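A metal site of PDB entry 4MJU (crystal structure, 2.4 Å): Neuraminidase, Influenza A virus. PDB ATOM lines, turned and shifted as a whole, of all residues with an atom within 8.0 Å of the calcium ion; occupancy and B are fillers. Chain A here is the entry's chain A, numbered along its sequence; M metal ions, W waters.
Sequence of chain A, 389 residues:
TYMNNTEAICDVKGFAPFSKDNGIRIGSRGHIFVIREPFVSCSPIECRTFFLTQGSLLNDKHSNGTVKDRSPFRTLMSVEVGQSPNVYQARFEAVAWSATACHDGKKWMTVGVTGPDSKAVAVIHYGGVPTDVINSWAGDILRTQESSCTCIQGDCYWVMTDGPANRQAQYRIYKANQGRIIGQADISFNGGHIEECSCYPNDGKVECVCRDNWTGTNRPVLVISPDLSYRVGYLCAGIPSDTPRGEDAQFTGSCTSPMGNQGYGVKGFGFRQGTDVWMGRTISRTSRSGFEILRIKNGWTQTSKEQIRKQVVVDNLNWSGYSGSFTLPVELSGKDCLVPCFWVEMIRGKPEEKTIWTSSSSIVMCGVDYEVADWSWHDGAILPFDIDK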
ATOM      1  N   HIS A 193      24.237 -28.405 -10.328  1.00  0.00           N
ATOM      2  CA  HIS A 193      25.405 -28.994 -10.965  1.00  0.00           C
ATOM      3  C   HIS A 193      26.662 -28.778 -10.120  1.00  0.00           C
ATOM      4  O   HIS A 193      26.937 -27.650  -9.698  1.00  0.00           O
ATOM      5  CB  HIS A 193      25.595 -28.390 -12.360  1.00  0.00           C
ATOM      6  CG  HIS A 193      26.424 -29.230 -13.275  1.00  0.00           C
ATOM      7  ND1 HIS A 193      27.726 -28.914 -13.612  1.00  0.00           N
ATOM      8  CD2 HIS A 193      26.140 -30.390 -13.908  1.00  0.00           C
ATOM      9  CE1 HIS A 193      28.195 -29.834 -14.435  1.00  0.00           C
ATOM     10  NE2 HIS A 193      27.257 -30.743 -14.617  1.00  0.00           N
ATOM     11  N   CYS A 210      31.877 -24.593  -5.303  1.00  0.00           N
ATOM     12  CA  CYS A 210      32.139 -25.389  -6.490  1.00  0.00           C
ATOM     13  C   CYS A 210      31.800 -24.664  -7.784  1.00  0.00           C
ATOM     14  O   CYS A 210      31.680 -23.432  -7.816  1.00  0.00           O
ATOM     15  CB  CYS A 210      31.417 -26.730  -6.376  1.00  0.00           C
ATOM     16  SG  CYS A 210      31.618 -27.552  -4.759  1.00  0.00           S
ATOM     17  N   ARG A 211      31.686 -25.426  -8.857  1.00  0.00           N
ATOM     18  CA  ARG A 211      31.434 -24.886 -10.185  1.00  0.00           C
ATOM     19  C   ARG A 211      30.200 -25.564 -10.784  1.00  0.00           C
ATOM     20  O   ARG A 211      30.155 -26.796 -10.918  1.00  0.00           O
ATOM     21  CB  ARG A 211      32.661 -25.101 -11.072  1.00  0.00           C
ATOM     22  CG  ARG A 211      32.432 -24.939 -12.580  1.00  0.00           C
ATOM     23  CD  ARG A 211      33.696 -25.315 -13.364  1.00  0.00           C
ATOM     24  NE  ARG A 211      33.503 -25.333 -14.806  1.00  0.00           N
ATOM     25  CZ  ARG A 211      34.493 -25.507 -15.698  1.00  0.00           C
ATOM     26  NH1 ARG A 211      34.222 -25.498 -17.004  1.00  0.00           N
ATOM     27  NH2 ARG A 211      35.746 -25.694 -15.285  1.00  0.00           N
ATOM     28  N   ASP A 212      29.184 -24.754 -11.103  1.00  0.00           N
ATOM     29  CA  ASP A 212      28.034 -25.201 -11.856  1.00  0.00           C
ATOM     30  C   ASP A 212      28.333 -24.965 -13.325  1.00  0.00           C
ATOM     31  O   ASP A 212      28.518 -23.821 -13.757  1.00  0.00           O
ATOM     32  CB  ASP A 212      26.767 -24.444 -11.423  1.00  0.00           C
ATOM     33  CG  ASP A 212      25.505 -24.877 -12.185  1.00  0.00           C
ATOM     34  OD1 ASP A 212      24.454 -25.050 -11.526  1.00  0.00           O
ATOM     35  OD2 ASP A 212      25.534 -25.002 -13.423  1.00  0.00           O
ATOM     36  N   ASN A 213      28.383 -26.047 -14.085  1.00  0.00           N
ATOM     37  CA  ASN A 213      28.735 -25.976 -15.491  1.00  0.00           C
ATOM     38  C   ASN A 213      27.507 -26.117 -16.395  1.00  0.00           C
ATOM     39  O   ASN A 213      27.628 -26.236 -17.610  1.00  0.00           O
ATOM     40  CB  ASN A 213      29.763 -27.084 -15.813  1.00  0.00           C
ATOM     41  CG  ASN A 213      30.735 -26.669 -16.902  1.00  0.00           C
ATOM     42  OD1 ASN A 213      31.337 -25.607 -16.839  1.00  0.00           O
ATOM     43  ND2 ASN A 213      30.878 -27.516 -17.929  1.00  0.00           N
ATOM     44  N   TRP A 214      26.337 -26.064 -15.778  1.00  0.00           N
ATOM     45  CA  TRP A 214      25.053 -26.328 -16.430  1.00  0.00           C
ATOM     46  C   TRP A 214      24.304 -25.015 -16.709  1.00  0.00           C
ATOM     47  O   TRP A 214      24.195 -24.590 -17.855  1.00  0.00           O
ATOM     48  CB  TRP A 214      24.197 -27.238 -15.535  1.00  0.00           C
ATOM     49  CG  TRP A 214      22.950 -27.805 -16.156  1.00  0.00           C
ATOM     50  CD1 TRP A 214      22.513 -27.636 -17.445  1.00  0.00           C
ATOM     51  CD2 TRP A 214      21.980 -28.652 -15.528  1.00  0.00           C
ATOM     52  NE1 TRP A 214      21.341 -28.317 -17.640  1.00  0.00           N
ATOM     53  CE2 TRP A 214      20.987 -28.944 -16.480  1.00  0.00           C
ATOM     54  CE3 TRP A 214      21.870 -29.197 -14.232  1.00  0.00           C
ATOM     55  CZ2 TRP A 214      19.889 -29.753 -16.180  1.00  0.00           C
ATOM     56  CZ3 TRP A 214      20.768 -29.992 -13.950  1.00  0.00           C
ATOM     57  CH2 TRP A 214      19.792 -30.267 -14.916  1.00  0.00           C
ATOM     58  N   THR A 215      23.787 -24.391 -15.653  1.00  0.00           N
ATOM     59  CA  THR A 215      23.041 -23.142 -15.793  1.00  0.00           C
ATOM     60  C   THR A 215      23.435 -22.030 -14.796  1.00  0.00           C
ATOM     61  O   THR A 215      22.934 -20.903 -14.891  1.00  0.00           O
ATOM     62  CB  THR A 215      21.528 -23.362 -15.630  1.00  0.00           C
ATOM     63  OG1 THR A 215      21.241 -23.610 -14.247  1.00  0.00           O
ATOM     64  CG2 THR A 215      21.040 -24.526 -16.496  1.00  0.00           C
ATOM     65  N   GLY A 216      24.296 -22.333 -13.844  1.00  0.00           N
ATOM     66  CA  GLY A 216      24.566 -21.406 -12.757  1.00  0.00           C
ATOM     67  C   GLY A 216      25.774 -20.521 -12.980  1.00  0.00           C
ATOM     68  O   GLY A 216      26.841 -21.010 -13.347  1.00  0.00           O
ATOM     69  N   THR A 217      25.606 -19.223 -12.747  1.00  0.00           N
ATOM     70  CA  THR A 217      26.720 -18.266 -12.730  1.00  0.00           C
ATOM     71  C   THR A 217      27.027 -17.903 -11.290  1.00  0.00           C
ATOM     72  O   THR A 217      28.021 -17.218 -10.998  1.00  0.00           O
ATOM     73  CB  THR A 217      26.429 -16.984 -13.531  1.00  0.00           C
ATOM     74  OG1 THR A 217      25.415 -16.224 -12.848  1.00  0.00           O
ATOM     75  CG2 THR A 217      25.934 -17.327 -14.923  1.00  0.00           C
ATOM     76  N   ASN A 218      26.172 -18.345 -10.373  1.00  0.00           N
ATOM     77  CA  ASN A 218      26.551 -18.400  -8.974  1.00  0.00           C
ATOM     78  C   ASN A 218      27.127 -19.778  -8.692  1.00  0.00           C
ATOM     79  O   ASN A 218      26.932 -20.717  -9.470  1.00  0.00           O
ATOM     80  CB  ASN A 218      25.396 -18.087  -8.018  1.00  0.00           C
ATOM     81  CG  ASN A 218      24.138 -18.894  -8.333  1.00  0.00           C
ATOM     82  OD1 ASN A 218      24.101 -19.697  -9.273  1.00  0.00           O
ATOM     83  ND2 ASN A 218      23.104 -18.675  -7.527  1.00  0.00           N
ATOM     84  N   ARG A 219      27.819 -19.902  -7.560  1.00  0.00           N
ATOM     85  CA  ARG A 219      28.548 -21.120  -7.246  1.00  0.00           C
ATOM     86  C   ARG A 219      27.832 -21.990  -6.239  1.00  0.00           C
ATOM     87  O   ARG A 219      27.345 -21.503  -5.230  1.00  0.00           O
ATOM     88  CB  ARG A 219      29.955 -20.776  -6.755  1.00  0.00           C
ATOM     89  CG  ARG A 219      30.856 -20.186  -7.833  1.00  0.00           C
ATOM     90  CD  ARG A 219      32.306 -20.267  -7.399  1.00  0.00           C
ATOM     91  NE  ARG A 219      33.209 -19.717  -8.394  1.00  0.00           N
ATOM     92  CZ  ARG A 219      33.642 -20.385  -9.451  1.00  0.00           C
ATOM     93  NH1 ARG A 219      34.488 -19.804 -10.307  1.00  0.00           N
ATOM     94  NH2 ARG A 219      33.242 -21.634  -9.650  1.00  0.00           N
ATOM     95  N   PRO A 220      27.760 -23.292  -6.522  1.00  0.00           N
ATOM     96  CA  PRO A 220      27.165 -24.178  -5.527  1.00  0.00           C
ATOM     97  C   PRO A 220      28.020 -24.285  -4.267  1.00  0.00           C
ATOM     98  O   PRO A 220      29.246 -24.114  -4.319  1.00  0.00           O
ATOM     99  CB  PRO A 220      27.022 -25.519  -6.249  1.00  0.00           C
ATOM    100  CG  PRO A 220      27.750 -25.387  -7.521  1.00  0.00           C
ATOM    101  CD  PRO A 220      27.947 -23.956  -7.826  1.00  0.00           C
ATOM    102  N   SER A 241      29.908 -15.141  -9.236  1.00  0.00           N
ATOM    103  CA  SER A 241      31.372 -15.233  -9.286  1.00  0.00           C
ATOM    104  C   SER A 241      31.922 -16.346 -10.187  1.00  0.00           C
ATOM    105  O   SER A 241      33.107 -16.697 -10.092  1.00  0.00           O
ATOM    106  CB  SER A 241      31.979 -15.286  -7.870  1.00  0.00           C
ATOM    107  OG  SER A 241      31.558 -16.433  -7.152  1.00  0.00           O
ATOM    108  N   ASP A 242      31.093 -16.881 -11.076  1.00  0.00           N
ATOM    109  CA  ASP A 242      31.589 -17.850 -12.067  1.00  0.00           C
ATOM    110  C   ASP A 242      31.913 -17.091 -13.359  1.00  0.00           C
ATOM    111  O   ASP A 242      31.667 -15.882 -13.465  1.00  0.00           O
ATOM    112  CB  ASP A 242      30.570 -18.987 -12.304  1.00  0.00           C
ATOM    113  CG  ASP A 242      31.189 -20.216 -12.990  1.00  0.00           C
ATOM    114  OD1 ASP A 242      30.444 -21.185 -13.263  1.00  0.00           O
ATOM    115  OD2 ASP A 242      32.408 -20.222 -13.241  1.00  0.00           O
ATOM    116  N   THR A 243      32.464 -17.793 -14.340  1.00  0.00           N
ATOM    117  CA  THR A 243      32.829 -17.200 -15.614  1.00  0.00           C
ATOM    118  C   THR A 243      32.590 -18.230 -16.716  1.00  0.00           C
ATOM    119  O   THR A 243      33.181 -19.298 -16.677  1.00  0.00           O
ATOM    120  CB  THR A 243      34.325 -16.800 -15.631  1.00  0.00           C
ATOM    121  OG1 THR A 243      34.602 -15.923 -14.527  1.00  0.00           O
ATOM    122  CG2 THR A 243      34.696 -16.129 -16.944  1.00  0.00           C
ATOM    123  N   PRO A 244      31.743 -17.904 -17.723  1.00  0.00           N
ATOM    124  CA  PRO A 244      31.106 -16.605 -17.993  1.00  0.00           C
ATOM    125  C   PRO A 244      29.951 -16.301 -17.061  1.00  0.00           C
ATOM    126  O   PRO A 244      29.483 -17.217 -16.375  1.00  0.00           O
ATOM    127  CB  PRO A 244      30.563 -16.786 -19.417  1.00  0.00           C
ATOM    128  CG  PRO A 244      30.214 -18.230 -19.479  1.00  0.00           C
ATOM    129  CD  PRO A 244      31.269 -18.939 -18.654  1.00  0.00           C
ATOM    130  N   ARG A 245      29.517 -15.035 -17.045  1.00  0.00           N
ATOM    131  CA  ARG A 245      28.466 -14.558 -16.155  1.00  0.00           C
ATOM    132  C   ARG A 245      27.967 -13.196 -16.632  1.00  0.00           C
ATOM    133  O   ARG A 245      28.578 -12.561 -17.489  1.00  0.00           O
ATOM    134  CB  ARG A 245      28.979 -14.433 -14.709  1.00  0.00           C
ATOM    135  CG  ARG A 245      29.871 -13.197 -14.510  1.00  0.00           C
ATOM    136  CD  ARG A 245      30.381 -13.045 -13.077  1.00  0.00           C
ATOM    137  NE  ARG A 245      31.356 -11.954 -12.994  1.00  0.00           N
ATOM    138  CZ  ARG A 245      32.668 -12.088 -13.073  1.00  0.00           C
ATOM    139  NH1 ARG A 245      33.446 -11.017 -12.977  1.00  0.00           N
ATOM    140  NH2 ARG A 245      33.235 -13.293 -13.235  1.00  0.00           N
ATOM    141  N   MET A 259      21.351 -19.403 -10.578  1.00  0.00           N
ATOM    142  CA  MET A 259      20.846 -18.185 -11.213  1.00  0.00           C
ATOM    143  C   MET A 259      21.775 -17.797 -12.346  1.00  0.00           C
ATOM    144  O   MET A 259      22.932 -18.214 -12.368  1.00  0.00           O
ATOM    145  CB  MET A 259      20.754 -17.046 -10.190  1.00  0.00           C
ATOM    146  CG  MET A 259      19.916 -17.391  -8.960  1.00  0.00           C
ATOM    147  SD  MET A 259      18.142 -17.511  -9.332  1.00  0.00           S
ATOM    148  CE  MET A 259      17.706 -15.769  -9.346  1.00  0.00           C
ATOM    149  N   ASN A 261      21.242 -18.342 -15.730  1.00  0.00           N
ATOM    150  CA  ASN A 261      20.955 -19.099 -16.957  1.00  0.00           C
ATOM    151  C   ASN A 261      22.048 -19.008 -18.022  1.00  0.00           C
ATOM    152  O   ASN A 261      21.825 -18.502 -19.126  1.00  0.00           O
ATOM    153  CB  ASN A 261      19.595 -18.676 -17.544  1.00  0.00           C
ATOM    154  CG  ASN A 261      19.132 -19.613 -18.655  1.00  0.00           C
ATOM    155  OD1 ASN A 261      19.629 -20.738 -18.790  1.00  0.00           O
ATOM    156  ND2 ASN A 261      18.180 -19.150 -19.466  1.00  0.00           N
ATOM    157  N   GLN A 262      23.242 -19.470 -17.665  1.00  0.00           N
ATOM    158  CA  GLN A 262      24.347 -19.499 -18.607  1.00  0.00           C
ATOM    159  C   GLN A 262      25.069 -20.821 -18.460  1.00  0.00           C
ATOM    160  O   GLN A 262      25.092 -21.386 -17.364  1.00  0.00           O
ATOM    161  CB  GLN A 262      25.333 -18.348 -18.380  1.00  0.00           C
ATOM    162  CG  GLN A 262      24.932 -17.044 -19.019  1.00  0.00           C
ATOM    163  CD  GLN A 262      25.977 -15.975 -18.862  1.00  0.00           C
ATOM    164  OE1 GLN A 262      25.876 -15.116 -17.984  1.00  0.00           O
ATOM    165  NE2 GLN A 262      27.016 -16.014 -19.699  1.00  0.00           N
ATOM    166  N   GLY A 263      25.648 -21.307 -19.552  1.00  0.00           N
ATOM    167  CA  GLY A 263      26.412 -22.533 -19.519  1.00  0.00           C
ATOM    168  C   GLY A 263      27.863 -22.260 -19.149  1.00  0.00           C
ATOM    169  O   GLY A 263      28.246 -21.127 -18.828  1.00  0.00           O
ATOM    170  N   TYR A 264      28.676 -23.313 -19.186  1.00  0.00           N
ATOM    171  CA  TYR A 264      30.098 -23.203 -18.908  1.00  0.00           C
ATOM    172  C   TYR A 264      30.374 -22.801 -17.461  1.00  0.00           C
ATOM    173  O   TYR A 264      29.471 -22.769 -16.622  1.00  0.00           O
ATOM    174  CB  TYR A 264      30.747 -22.204 -19.853  1.00  0.00           C
ATOM    175  CG  TYR A 264      32.204 -22.512 -20.166  1.00  0.00           C
ATOM    176  CD1 TYR A 264      32.578 -23.772 -20.595  1.00  0.00           C
ATOM    177  CD2 TYR A 264      33.183 -21.544 -20.045  1.00  0.00           C
ATOM    178  CE1 TYR A 264      33.900 -24.065 -20.887  1.00  0.00           C
ATOM    179  CE2 TYR A 264      34.500 -21.816 -20.331  1.00  0.00           C
ATOM    180  CZ  TYR A 264      34.857 -23.080 -20.743  1.00  0.00           C
ATOM    181  OH  TYR A 264      36.173 -23.365 -21.033  1.00  0.00           O
ATOM    182  N   GLY A 265      31.636 -22.495 -17.187  1.00  0.00           N
ATOM    183  CA  GLY A 265      32.087 -22.135 -15.857  1.00  0.00           C
ATOM    184  C   GLY A 265      33.601 -22.150 -15.763  1.00  0.00           C
ATOM    185  O   GLY A 265      34.302 -22.344 -16.757  1.00  0.00           O
ATOM    186  N   VAL A 266      34.110 -21.914 -14.558  1.00  0.00           N
ATOM    187  CA  VAL A 266      35.527 -22.019 -14.281  1.00  0.00           C
ATOM    188  C   VAL A 266      35.598 -22.445 -12.826  1.00  0.00           C
ATOM    189  O   VAL A 266      34.735 -22.067 -12.038  1.00  0.00           O
ATOM    190  CB  VAL A 266      36.266 -20.687 -14.543  1.00  0.00           C
ATOM    191  CG1 VAL A 266      35.761 -19.552 -13.630  1.00  0.00           C
ATOM    192  CG2 VAL A 266      37.798 -20.874 -14.424  1.00  0.00           C
HETATM  193 CA    CA M   1      28.800 -21.759 -14.779  1.00  0.00          CA
HETATM  194  O   HOH W   1      26.631 -23.157 -16.113  1.00  0.00           O
HETATM  195  O   HOH W   2      28.669 -20.012 -16.527  1.00  0.00           O
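The backbone carbonyl oxygen (O) of Tyr 264 binds the calcium ion (2.2 Å).
The side-chain carboxylate (OD1) of Asp 242 binds the calcium ion, 2.3 Å away.
The backbone carbonyl oxygen (O) of Asp 212 binds the calcium ion (2.3 Å).
The calcium ion is bound by water W2, 2.5 Å away.
The calcium ion is bound by the backbone carbonyl oxygen (O) of Gly 216 (2.5 Å).
Slightly farther from the calcium ion lies water W1 (2.9 Å).
Water W2 bridges the backbone carbonyl oxygen (O) of Gly 263 (2.6 Å) and the backbone carbonyl oxygen (O) of Pro 244 (2.9 Å).
The backbone carbonyl oxygen (O) of Asn 213 lies within hydrogen-bond range of the backbone NH (N) of Tyr 264 (3.5 Å).
N of Asp 242 is in hydrogen-bond range of O of Thr 217.
The side-chain carboxylate (OD2) of Asp 242 lies within hydrogen-bond range of the backbone NH (N) of Val 266 (2.7 Å).
The guanidinium group (NH1) of Arg 219 is in salt-bridge range of the side-chain carboxylate (OD2) of Asp 242 (3.6 Å).
NH2 of Arg 245 sits at hydrogen-bond distance from O of Asp 242, at 3.0 Å.
OD2 of Asp 212 sits at hydrogen-bond distance from N of Trp 214, at 2.7 Å.
The backbone NH (N) of Thr 215 lies within hydrogen-bond range of the side-chain carboxylate (OD2) of Asp 212 (2.9 Å).
The backbone carbonyl oxygen of Gly 265 lies within hydrogen-bond range of the guanidinium group of Arg 211 (3.2 Å).
Gly 265 touches the calcium ion (CA to CA, 3.5 Å).
Along chain A the residues within 4 Å of the calcium ion span positions 212 to 265.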
